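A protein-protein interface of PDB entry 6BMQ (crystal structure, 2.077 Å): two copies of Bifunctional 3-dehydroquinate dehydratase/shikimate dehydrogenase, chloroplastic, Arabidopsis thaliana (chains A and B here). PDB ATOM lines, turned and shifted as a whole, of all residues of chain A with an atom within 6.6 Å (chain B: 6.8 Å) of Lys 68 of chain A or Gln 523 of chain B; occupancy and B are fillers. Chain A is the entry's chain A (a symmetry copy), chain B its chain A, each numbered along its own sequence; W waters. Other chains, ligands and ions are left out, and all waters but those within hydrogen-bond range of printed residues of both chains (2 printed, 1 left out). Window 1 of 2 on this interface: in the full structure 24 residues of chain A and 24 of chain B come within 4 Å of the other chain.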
ATOM      1  N   ARG A  66     -21.660 -16.058   8.114  1.00  0.00           N
ATOM      2  CA  ARG A  66     -20.513 -15.289   7.650  1.00  0.00           C
ATOM      3  C   ARG A  66     -19.543 -16.101   6.790  1.00  0.00           C
ATOM      4  O   ARG A  66     -18.976 -17.098   7.250  1.00  0.00           O
ATOM      5  CB  ARG A  66     -19.752 -14.687   8.829  1.00  0.00           C
ATOM      6  CG  ARG A  66     -18.815 -13.537   8.435  1.00  0.00           C
ATOM      7  CD  ARG A  66     -19.573 -12.264   8.081  1.00  0.00           C
ATOM      8  NE  ARG A  66     -20.004 -11.544   9.280  1.00  0.00           N
ATOM      9  CZ  ARG A  66     -21.063 -10.746   9.342  1.00  0.00           C
ATOM     10  NH1 ARG A  66     -21.818 -10.568   8.265  1.00  0.00           N
ATOM     11  NH2 ARG A  66     -21.376 -10.134  10.485  1.00  0.00           N
ATOM     12  N   PRO A  67     -19.334 -15.651   5.542  1.00  0.00           N
ATOM     13  CA  PRO A  67     -18.464 -16.296   4.558  1.00  0.00           C
ATOM     14  C   PRO A  67     -16.981 -16.060   4.857  1.00  0.00           C
ATOM     15  O   PRO A  67     -16.637 -15.089   5.521  1.00  0.00           O
ATOM     16  CB  PRO A  67     -18.871 -15.616   3.254  1.00  0.00           C
ATOM     17  CG  PRO A  67     -19.225 -14.224   3.695  1.00  0.00           C
ATOM     18  CD  PRO A  67     -19.937 -14.417   5.008  1.00  0.00           C
ATOM     19  N   LYS A  68     -16.120 -16.941   4.362  1.00  0.00           N
ATOM     20  CA  LYS A  68     -14.676 -16.772   4.509  1.00  0.00           C
ATOM     21  C   LYS A  68     -14.177 -15.388   4.044  1.00  0.00           C
ATOM     22  O   LYS A  68     -13.253 -14.830   4.645  1.00  0.00           O
ATOM     23  CB  LYS A  68     -13.930 -17.867   3.733  1.00  0.00           C
ATOM     24  CG  LYS A  68     -12.999 -18.726   4.582  1.00  0.00           C
ATOM     25  CD  LYS A  68     -13.780 -19.635   5.531  1.00  0.00           C
ATOM     26  CE  LYS A  68     -12.917 -20.788   6.029  1.00  0.00           C
ATOM     27  NZ  LYS A  68     -13.684 -21.939   6.623  1.00  0.00           N
ATOM     28  N   TRP A  69     -14.778 -14.830   2.991  1.00  0.00           N
ATOM     29  CA  TRP A  69     -14.292 -13.555   2.452  1.00  0.00           C
ATOM     30  C   TRP A  69     -14.698 -12.339   3.298  1.00  0.00           C
ATOM     31  O   TRP A  69     -14.380 -11.202   2.954  1.00  0.00           O
ATOM     32  CB  TRP A  69     -14.748 -13.362   0.995  1.00  0.00           C
ATOM     33  CG  TRP A  69     -16.194 -13.711   0.676  1.00  0.00           C
ATOM     34  CD1 TRP A  69     -16.658 -14.889   0.164  1.00  0.00           C
ATOM     35  CD2 TRP A  69     -17.343 -12.855   0.810  1.00  0.00           C
ATOM     36  NE1 TRP A  69     -18.023 -14.834  -0.007  1.00  0.00           N
ATOM     37  CE2 TRP A  69     -18.468 -13.596   0.383  1.00  0.00           C
ATOM     38  CE3 TRP A  69     -17.533 -11.545   1.271  1.00  0.00           C
ATOM     39  CZ2 TRP A  69     -19.756 -13.072   0.401  1.00  0.00           C
ATOM     40  CZ3 TRP A  69     -18.813 -11.023   1.290  1.00  0.00           C
ATOM     41  CH2 TRP A  69     -19.908 -11.784   0.855  1.00  0.00           C
ATOM     42  N   GLU A  70     -15.377 -12.567   4.419  1.00  0.00           N
ATOM     43  CA  GLU A  70     -15.715 -11.456   5.299  1.00  0.00           C
ATOM     44  C   GLU A  70     -15.362 -11.833   6.742  1.00  0.00           C
ATOM     45  O   GLU A  70     -16.013 -11.412   7.707  1.00  0.00           O
ATOM     46  CB  GLU A  70     -17.199 -11.078   5.141  1.00  0.00           C
ATOM     47  CG  GLU A  70     -17.628  -9.773   5.828  1.00  0.00           C
ATOM     48  CD  GLU A  70     -17.182  -8.515   5.095  1.00  0.00           C
ATOM     49  OE1 GLU A  70     -17.394  -7.403   5.641  1.00  0.00           O
ATOM     50  OE2 GLU A  70     -16.633  -8.631   3.977  1.00  0.00           O
ATOM     51  N   GLY A  71     -14.320 -12.646   6.877  1.00  0.00           N
ATOM     52  CA  GLY A  71     -13.831 -13.028   8.184  1.00  0.00           C
ATOM     53  C   GLY A  71     -14.563 -14.183   8.850  1.00  0.00           C
ATOM     54  O   GLY A  71     -14.308 -14.487  10.014  1.00  0.00           O
ATOM     55  N   GLY A  72     -15.453 -14.847   8.125  1.00  0.00           N
ATOM     56  CA  GLY A  72     -16.254 -15.902   8.734  1.00  0.00           C
ATOM     57  C   GLY A  72     -15.739 -17.289   8.440  1.00  0.00           C
ATOM     58  O   GLY A  72     -14.624 -17.451   7.941  1.00  0.00           O
ATOM     59  N   GLN A  73     -16.568 -18.288   8.715  1.00  0.00           N
ATOM     60  CA  GLN A  73     -16.170 -19.678   8.551  1.00  0.00           C
ATOM     61  C   GLN A  73     -16.820 -20.384   7.363  1.00  0.00           C
ATOM     62  O   GLN A  73     -16.367 -21.449   6.955  1.00  0.00           O
ATOM     63  CB  GLN A  73     -16.486 -20.459   9.828  1.00  0.00           C
ATOM     64  CG  GLN A  73     -15.871 -19.866  11.082  1.00  0.00           C
ATOM     65  CD  GLN A  73     -14.355 -19.979  11.098  1.00  0.00           C
ATOM     66  OE1 GLN A  73     -13.806 -21.074  10.956  1.00  0.00           O
ATOM     67  NE2 GLN A  73     -13.670 -18.842  11.265  1.00  0.00           N
ATOM     68  N   TYR A  74     -17.875 -19.801   6.800  1.00  0.00           N
ATOM     69  CA  TYR A  74     -18.624 -20.487   5.754  1.00  0.00           C
ATOM     70  C   TYR A  74     -17.879 -20.528   4.432  1.00  0.00           C
ATOM     71  O   TYR A  74     -17.450 -19.493   3.912  1.00  0.00           O
ATOM     72  CB  TYR A  74     -19.994 -19.837   5.517  1.00  0.00           C
ATOM     73  CG  TYR A  74     -20.746 -20.462   4.352  1.00  0.00           C
ATOM     74  CD1 TYR A  74     -21.477 -21.637   4.519  1.00  0.00           C
ATOM     75  CD2 TYR A  74     -20.717 -19.881   3.081  1.00  0.00           C
ATOM     76  CE1 TYR A  74     -22.173 -22.210   3.461  1.00  0.00           C
ATOM     77  CE2 TYR A  74     -21.413 -20.454   2.011  1.00  0.00           C
ATOM     78  CZ  TYR A  74     -22.133 -21.617   2.215  1.00  0.00           C
ATOM     79  OH  TYR A  74     -22.815 -22.199   1.175  1.00  0.00           O
ATOM     80  N   GLU A  75     -17.766 -21.737   3.886  1.00  0.00           N
ATOM     81  CA  GLU A  75     -17.272 -21.963   2.535  1.00  0.00           C
ATOM     82  C   GLU A  75     -18.315 -22.742   1.748  1.00  0.00           C
ATOM     83  O   GLU A  75     -18.997 -23.601   2.299  1.00  0.00           O
ATOM     84  CB  GLU A  75     -15.955 -22.730   2.556  1.00  0.00           C
ATOM     85  CG  GLU A  75     -14.774 -21.869   2.910  1.00  0.00           C
ATOM     86  CD  GLU A  75     -13.477 -22.641   2.865  1.00  0.00           C
ATOM     87  OE1 GLU A  75     -12.514 -22.148   2.231  1.00  0.00           O
ATOM     88  OE2 GLU A  75     -13.433 -23.745   3.457  1.00  0.00           O
ATOM     89  N   GLY B 183      -2.909 -11.551   7.896  1.00  0.00           N
ATOM     90  CA  GLY B 183      -3.883 -10.809   7.112  1.00  0.00           C
ATOM     91  C   GLY B 183      -3.769 -11.209   5.655  1.00  0.00           C
ATOM     92  O   GLY B 183      -2.726 -11.740   5.246  1.00  0.00           O
ATOM     93  N   GLU B 184      -4.818 -10.958   4.866  1.00  0.00           N
ATOM     94  CA  GLU B 184      -4.777 -11.330   3.455  1.00  0.00           C
ATOM     95  C   GLU B 184      -3.605 -10.661   2.754  1.00  0.00           C
ATOM     96  O   GLU B 184      -2.976 -11.274   1.893  1.00  0.00           O
ATOM     97  CB  GLU B 184      -6.085 -10.993   2.724  1.00  0.00           C
ATOM     98  CG  GLU B 184      -6.063 -11.460   1.261  1.00  0.00           C
ATOM     99  CD  GLU B 184      -7.321 -11.111   0.464  1.00  0.00           C
ATOM    100  OE1 GLU B 184      -8.347 -10.758   1.086  1.00  0.00           O
ATOM    101  OE2 GLU B 184      -7.271 -11.198  -0.795  1.00  0.00           O
ATOM    102  N   ARG B 185      -3.287  -9.421   3.137  1.00  0.00           N
ATOM    103  CA  ARG B 185      -2.197  -8.690   2.483  1.00  0.00           C
ATOM    104  C   ARG B 185      -0.821  -9.227   2.860  1.00  0.00           C
ATOM    105  O   ARG B 185       0.173  -8.865   2.234  1.00  0.00           O
ATOM    106  CB  ARG B 185      -2.280  -7.182   2.807  1.00  0.00           C
ATOM    107  CG  ARG B 185      -3.371  -6.476   2.009  1.00  0.00           C
ATOM    108  CD  ARG B 185      -3.780  -5.139   2.634  1.00  0.00           C
ATOM    109  NE  ARG B 185      -4.773  -4.481   1.801  1.00  0.00           N
ATOM    110  CZ  ARG B 185      -6.061  -4.795   1.801  1.00  0.00           C
ATOM    111  NH1 ARG B 185      -6.520  -5.740   2.618  1.00  0.00           N
ATOM    112  NH2 ARG B 185      -6.889  -4.151   1.005  1.00  0.00           N
ATOM    113  N   LEU B 187      -0.272 -12.613   2.944  1.00  0.00           N
ATOM    114  CA  LEU B 187      -0.295 -14.034   2.550  1.00  0.00           C
ATOM    115  C   LEU B 187       1.009 -14.473   1.887  1.00  0.00           C
ATOM    116  O   LEU B 187       1.508 -15.564   2.133  1.00  0.00           O
ATOM    117  CB  LEU B 187      -1.462 -14.312   1.602  1.00  0.00           C
ATOM    118  CG  LEU B 187      -1.539 -15.743   1.035  1.00  0.00           C
ATOM    119  CD1 LEU B 187      -1.457 -16.784   2.129  1.00  0.00           C
ATOM    120  CD2 LEU B 187      -2.813 -15.938   0.224  1.00  0.00           C
ATOM    121  N   ASP B 206      -7.578 -27.590   7.115  1.00  0.00           N
ATOM    122  CA  ASP B 206      -8.515 -27.144   6.102  1.00  0.00           C
ATOM    123  C   ASP B 206      -8.881 -25.716   6.461  1.00  0.00           C
ATOM    124  O   ASP B 206      -8.535 -25.252   7.539  1.00  0.00           O
ATOM    125  CB  ASP B 206      -9.750 -28.035   6.044  1.00  0.00           C
ATOM    126  CG  ASP B 206     -10.376 -28.226   7.397  1.00  0.00           C
ATOM    127  OD1 ASP B 206     -10.379 -29.376   7.891  1.00  0.00           O
ATOM    128  OD2 ASP B 206     -10.837 -27.217   7.977  1.00  0.00           O
ATOM    129  N   SER B 207      -9.609 -25.038   5.584  1.00  0.00           N
ATOM    130  CA  SER B 207      -9.864 -23.606   5.750  1.00  0.00           C
ATOM    131  C   SER B 207     -10.663 -23.239   7.009  1.00  0.00           C
ATOM    132  O   SER B 207     -10.566 -22.111   7.496  1.00  0.00           O
ATOM    133  CB  SER B 207     -10.585 -23.070   4.521  1.00  0.00           C
ATOM    134  OG  SER B 207     -10.165 -23.756   3.350  1.00  0.00           O
ATOM    135  N   SER B 208     -11.431 -24.180   7.554  1.00  0.00           N
ATOM    136  CA  SER B 208     -12.200 -23.897   8.768  1.00  0.00           C
ATOM    137  C   SER B 208     -11.294 -23.851  10.011  1.00  0.00           C
ATOM    138  O   SER B 208     -11.688 -23.346  11.067  1.00  0.00           O
ATOM    139  CB  SER B 208     -13.321 -24.935   8.956  1.00  0.00           C
ATOM    140  OG  SER B 208     -12.811 -26.244   9.184  1.00  0.00           O
ATOM    141  N   LYS B 209     -10.071 -24.357   9.879  1.00  0.00           N
ATOM    142  CA  LYS B 209      -9.195 -24.488  11.040  1.00  0.00           C
ATOM    143  C   LYS B 209      -7.998 -23.532  10.994  1.00  0.00           C
ATOM    144  O   LYS B 209      -6.841 -23.975  11.066  1.00  0.00           O
ATOM    145  CB  LYS B 209      -8.717 -25.938  11.166  1.00  0.00           C
ATOM    146  CG  LYS B 209      -9.884 -26.928  11.220  1.00  0.00           C
ATOM    147  CD  LYS B 209      -9.414 -28.361  11.380  1.00  0.00           C
ATOM    148  CE  LYS B 209     -10.600 -29.315  11.499  1.00  0.00           C
ATOM    149  NZ  LYS B 209     -10.162 -30.666  11.942  1.00  0.00           N
ATOM    150  N   VAL B 210      -8.293 -22.230  10.891  1.00  0.00           N
ATOM    151  CA  VAL B 210      -7.277 -21.169  10.886  1.00  0.00           C
ATOM    152  C   VAL B 210      -6.942 -20.677  12.314  1.00  0.00           C
ATOM    153  O   VAL B 210      -7.842 -20.348  13.079  1.00  0.00           O
ATOM    154  CB  VAL B 210      -7.747 -19.973  10.016  1.00  0.00           C
ATOM    155  CG1 VAL B 210      -6.977 -18.712  10.352  1.00  0.00           C
ATOM    156  CG2 VAL B 210      -7.627 -20.300   8.523  1.00  0.00           C
ATOM    157  N   PRO B 213      -4.972 -15.013  11.108  1.00  0.00           N
ATOM    158  CA  PRO B 213      -5.473 -14.547   9.796  1.00  0.00           C
ATOM    159  C   PRO B 213      -4.514 -14.751   8.611  1.00  0.00           C
ATOM    160  O   PRO B 213      -3.333 -14.438   8.723  1.00  0.00           O
ATOM    161  CB  PRO B 213      -5.711 -13.049  10.029  1.00  0.00           C
ATOM    162  CG  PRO B 213      -5.986 -12.936  11.493  1.00  0.00           C
ATOM    163  CD  PRO B 213      -5.095 -13.971  12.147  1.00  0.00           C
ATOM    164  N   GLY B 214      -5.031 -15.278   7.503  1.00  0.00           N
ATOM    165  CA  GLY B 214      -4.260 -15.422   6.275  1.00  0.00           C
ATOM    166  C   GLY B 214      -3.597 -16.774   5.984  1.00  0.00           C
ATOM    167  O   GLY B 214      -3.028 -16.959   4.916  1.00  0.00           O
ATOM    168  N   GLN B 215      -3.654 -17.713   6.919  1.00  0.00           N
ATOM    169  CA  GLN B 215      -2.995 -19.006   6.709  1.00  0.00           C
ATOM    170  C   GLN B 215      -3.645 -19.776   5.555  1.00  0.00           C
ATOM    171  O   GLN B 215      -4.865 -19.911   5.523  1.00  0.00           O
ATOM    172  CB  GLN B 215      -3.049 -19.853   7.975  1.00  0.00           C
ATOM    173  CG  GLN B 215      -2.338 -19.261   9.187  1.00  0.00           C
ATOM    174  CD  GLN B 215      -2.691 -20.001  10.468  1.00  0.00           C
ATOM    175  OE1 GLN B 215      -3.712 -20.686  10.534  1.00  0.00           O
ATOM    176  NE2 GLN B 215      -1.848 -19.865  11.493  1.00  0.00           N
ATOM    177  N   PRO B 216      -2.829 -20.272   4.609  1.00  0.00           N
ATOM    178  CA  PRO B 216      -3.348 -21.135   3.548  1.00  0.00           C
ATOM    179  C   PRO B 216      -3.511 -22.560   4.069  1.00  0.00           C
ATOM    180  O   PRO B 216      -3.107 -22.834   5.191  1.00  0.00           O
ATOM    181  CB  PRO B 216      -2.262 -21.053   2.472  1.00  0.00           C
ATOM    182  CG  PRO B 216      -1.000 -20.887   3.240  1.00  0.00           C
ATOM    183  CD  PRO B 216      -1.367 -20.100   4.504  1.00  0.00           C
ATOM    184  N   TYR B 225       0.901 -23.945  -4.607  1.00  0.00           N
ATOM    185  CA  TYR B 225       2.045 -23.042  -4.636  1.00  0.00           C
ATOM    186  C   TYR B 225       3.367 -23.785  -4.755  1.00  0.00           C
ATOM    187  O   TYR B 225       4.418 -23.143  -4.759  1.00  0.00           O
ATOM    188  CB  TYR B 225       2.085 -22.163  -3.378  1.00  0.00           C
ATOM    189  CG  TYR B 225       0.871 -21.279  -3.178  1.00  0.00           C
ATOM    190  CD1 TYR B 225      -0.033 -21.524  -2.138  1.00  0.00           C
ATOM    191  CD2 TYR B 225       0.607 -20.220  -4.038  1.00  0.00           C
ATOM    192  CE1 TYR B 225      -1.158 -20.716  -1.945  1.00  0.00           C
ATOM    193  CE2 TYR B 225      -0.517 -19.404  -3.858  1.00  0.00           C
ATOM    194  CZ  TYR B 225      -1.391 -19.658  -2.802  1.00  0.00           C
ATOM    195  OH  TYR B 225      -2.491 -18.859  -2.616  1.00  0.00           O
ATOM    196  N   SER B 245      -8.572 -12.476  -4.569  1.00  0.00           N
ATOM    197  CA  SER B 245      -8.718 -13.770  -3.933  1.00  0.00           C
ATOM    198  C   SER B 245      -9.447 -14.796  -4.807  1.00  0.00           C
ATOM    199  O   SER B 245      -9.435 -15.988  -4.510  1.00  0.00           O
ATOM    200  CB  SER B 245      -9.470 -13.630  -2.604  1.00  0.00           C
ATOM    201  OG  SER B 245     -10.773 -13.130  -2.846  1.00  0.00           O
ATOM    202  N   HIS B 268      -0.807 -14.674  -5.192  1.00  0.00           N
ATOM    203  CA  HIS B 268      -1.735 -13.558  -5.187  1.00  0.00           C
ATOM    204  C   HIS B 268      -1.074 -12.309  -4.631  1.00  0.00           C
ATOM    205  O   HIS B 268      -0.368 -12.379  -3.631  1.00  0.00           O
ATOM    206  CB  HIS B 268      -2.971 -13.889  -4.364  1.00  0.00           C
ATOM    207  CG  HIS B 268      -3.798 -14.985  -4.950  1.00  0.00           C
ATOM    208  ND1 HIS B 268      -3.582 -16.311  -4.644  1.00  0.00           N
ATOM    209  CD2 HIS B 268      -4.832 -14.958  -5.817  1.00  0.00           C
ATOM    210  CE1 HIS B 268      -4.453 -17.055  -5.304  1.00  0.00           C
ATOM    211  NE2 HIS B 268      -5.228 -16.259  -6.015  1.00  0.00           N
ATOM    212  N   TYR B 521     -11.723 -19.040  -2.508  1.00  0.00           N
ATOM    213  CA  TYR B 521     -11.078 -17.782  -2.180  1.00  0.00           C
ATOM    214  C   TYR B 521      -9.714 -18.073  -1.596  1.00  0.00           C
ATOM    215  O   TYR B 521      -9.582 -18.867  -0.669  1.00  0.00           O
ATOM    216  CB  TYR B 521     -11.937 -16.978  -1.216  1.00  0.00           C
ATOM    217  CG  TYR B 521     -13.256 -16.555  -1.835  1.00  0.00           C
ATOM    218  CD1 TYR B 521     -14.341 -17.425  -1.873  1.00  0.00           C
ATOM    219  CD2 TYR B 521     -13.409 -15.291  -2.384  1.00  0.00           C
ATOM    220  CE1 TYR B 521     -15.538 -17.046  -2.441  1.00  0.00           C
ATOM    221  CE2 TYR B 521     -14.598 -14.898  -2.952  1.00  0.00           C
ATOM    222  CZ  TYR B 521     -15.664 -15.780  -2.982  1.00  0.00           C
ATOM    223  OH  TYR B 521     -16.865 -15.388  -3.548  1.00  0.00           O
ATOM    224  N   PHE B 522      -8.697 -17.437  -2.164  1.00  0.00           N
ATOM    225  CA  PHE B 522      -7.338 -17.584  -1.678  1.00  0.00           C
ATOM    226  C   PHE B 522      -6.948 -16.335  -0.898  1.00  0.00           C
ATOM    227  O   PHE B 522      -6.629 -15.305  -1.476  1.00  0.00           O
ATOM    228  CB  PHE B 522      -6.401 -17.838  -2.850  1.00  0.00           C
ATOM    229  CG  PHE B 522      -6.793 -19.036  -3.661  1.00  0.00           C
ATOM    230  CD1 PHE B 522      -7.556 -18.892  -4.819  1.00  0.00           C
ATOM    231  CD2 PHE B 522      -6.468 -20.315  -3.226  1.00  0.00           C
ATOM    232  CE1 PHE B 522      -7.950 -20.018  -5.558  1.00  0.00           C
ATOM    233  CE2 PHE B 522      -6.862 -21.437  -3.949  1.00  0.00           C
ATOM    234  CZ  PHE B 522      -7.592 -21.288  -5.118  1.00  0.00           C
ATOM    235  N   GLN B 523      -7.006 -16.427   0.424  1.00  0.00           N
ATOM    236  CA  GLN B 523      -6.888 -15.234   1.262  1.00  0.00           C
ATOM    237  C   GLN B 523      -6.580 -15.532   2.727  1.00  0.00           C
ATOM    238  O   GLN B 523      -6.427 -16.683   3.147  1.00  0.00           O
ATOM    239  CB  GLN B 523      -8.179 -14.424   1.191  1.00  0.00           C
ATOM    240  CG  GLN B 523      -9.361 -15.089   1.858  1.00  0.00           C
ATOM    241  CD  GLN B 523     -10.571 -14.184   1.849  1.00  0.00           C
ATOM    242  OE1 GLN B 523     -11.364 -14.201   0.908  1.00  0.00           O
ATOM    243  NE2 GLN B 523     -10.695 -13.349   2.881  1.00  0.00           N
ATOM    244  OXT GLN B 523      -6.495 -14.597   3.529  1.00  0.00           O
HETATM  245  O   HOH W   1     -10.734 -19.341   2.250  1.00  0.00           O
HETATM  246  O   HOH W   2     -11.953 -21.057  -0.200  1.00  0.00           O
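Water W2 bridges the side-chain carboxylate of Glu 75 of chain A (2.7 Å) and the backbone NH of Tyr 521 of chain B (3.1 Å). Water W1 lies within hydrogen-bond range of the backbone carbonyl oxygen (O) of Tyr 521 of chain B (3.2 Å) and the side-chain carboxylate (OE1) of Glu 75 of chain A (3.3 Å).
No position is printed for both chains.
Trp 69 of chain A touches Tyr 521 of chain B. Trp 69 of chain A touches Gln 523 of chain B.
Printed residues of chain B within 4 Å of Trp 69 of chain A: Tyr 521 (3.4 Å) and Gln 523 (3.4 Å). Printed residues of chain B within 4 Å of Glu 75 of chain A: Ser 207 (3.1 Å). Gly 183 of chain B touches none of the printed residues of chain A. Arg 185 of chain B touches none of the printed residues of chain A. Of the printed residues of chain A, Ser 207 of chain B touches Lys 68 (3.1 Å) and Glu 75 (3.1 Å). Of the printed residues of chain A, Ser 208 of chain B touches Lys 68 and Gln 73. Printed residues of chain A within 4 Å of Tyr 521 of chain B: Trp 69. Of chain A, only Lys 68 (3.4 Å) and Trp 69 (3.4 Å) come within 4 Å of Gln 523 of chain B. The nearest printed residue of chain B that does not touch Lys 68 of chain A is Tyr 521 of chain B (5.4 Å). The nearest residue of chain A that does not touch Gln 523 of chain B is Glu 70 of chain A (5.0 Å).
Hydrophobic or aromatic side chains of chain B that line the printed part of chain A: Tyr 521. Of the 10 printed residues of chain A, 4 touch a printed residue of chain B. Hydrophobic or aromatic side chains of chain A that line the printed part of chain B: Trp 69. Among the printed residues, 7 pairs touch across the chains.
The side-chain carboxylate (OD2) of Asp 206 of chain B sits at hydrogen-bond distance from the side-chain hydroxyl (OG) of Ser 208 of chain B (2.5 Å). O of Arg 66 of chain A lies within hydrogen-bond range of N of Gln 73 of chain A (3.1 Å). The side-chain amino group (NZ) of Lys 68 of chain A sits at hydrogen-bond distance from the backbone carbonyl oxygen (O) of Gln 73 of chain A (2.7 Å). O of Tyr 74 of chain A sits at hydrogen-bond distance from N of Lys 68 of chain A (2.9 Å). The side-chain amino group of Lys 68 of chain A is in salt-bridge range of the side-chain carboxylate of Glu 75 of chain A, 3.7 Å away.
The backbone carbonyl oxygen (O) of Ser 207 of chain B lies close to the side-chain amino group (NZ) of Lys 68 of chain A, 3.2 Å away. The side-chain hydroxyl (OG) of Ser 207 of chain B is in hydrogen-bond range of the side-chain carboxylate (OE1) of Glu 75 of chain A, 3.1 Å away. The side-chain amide oxygen (OE1) of Gln 73 of chain A lies close to the backbone carbonyl oxygen (O) of Ser 208 of chain B (3.1 Å). The backbone carbonyl oxygen of Lys 68 of chain A lies within hydrogen-bond range of the side-chain amide nitrogen of Gln 523 of chain B (3.4 Å). The side-chain amino group of Lys 68 of chain A lies close to the backbone NH of Ser 208 of chain B, at 3.3 Å.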
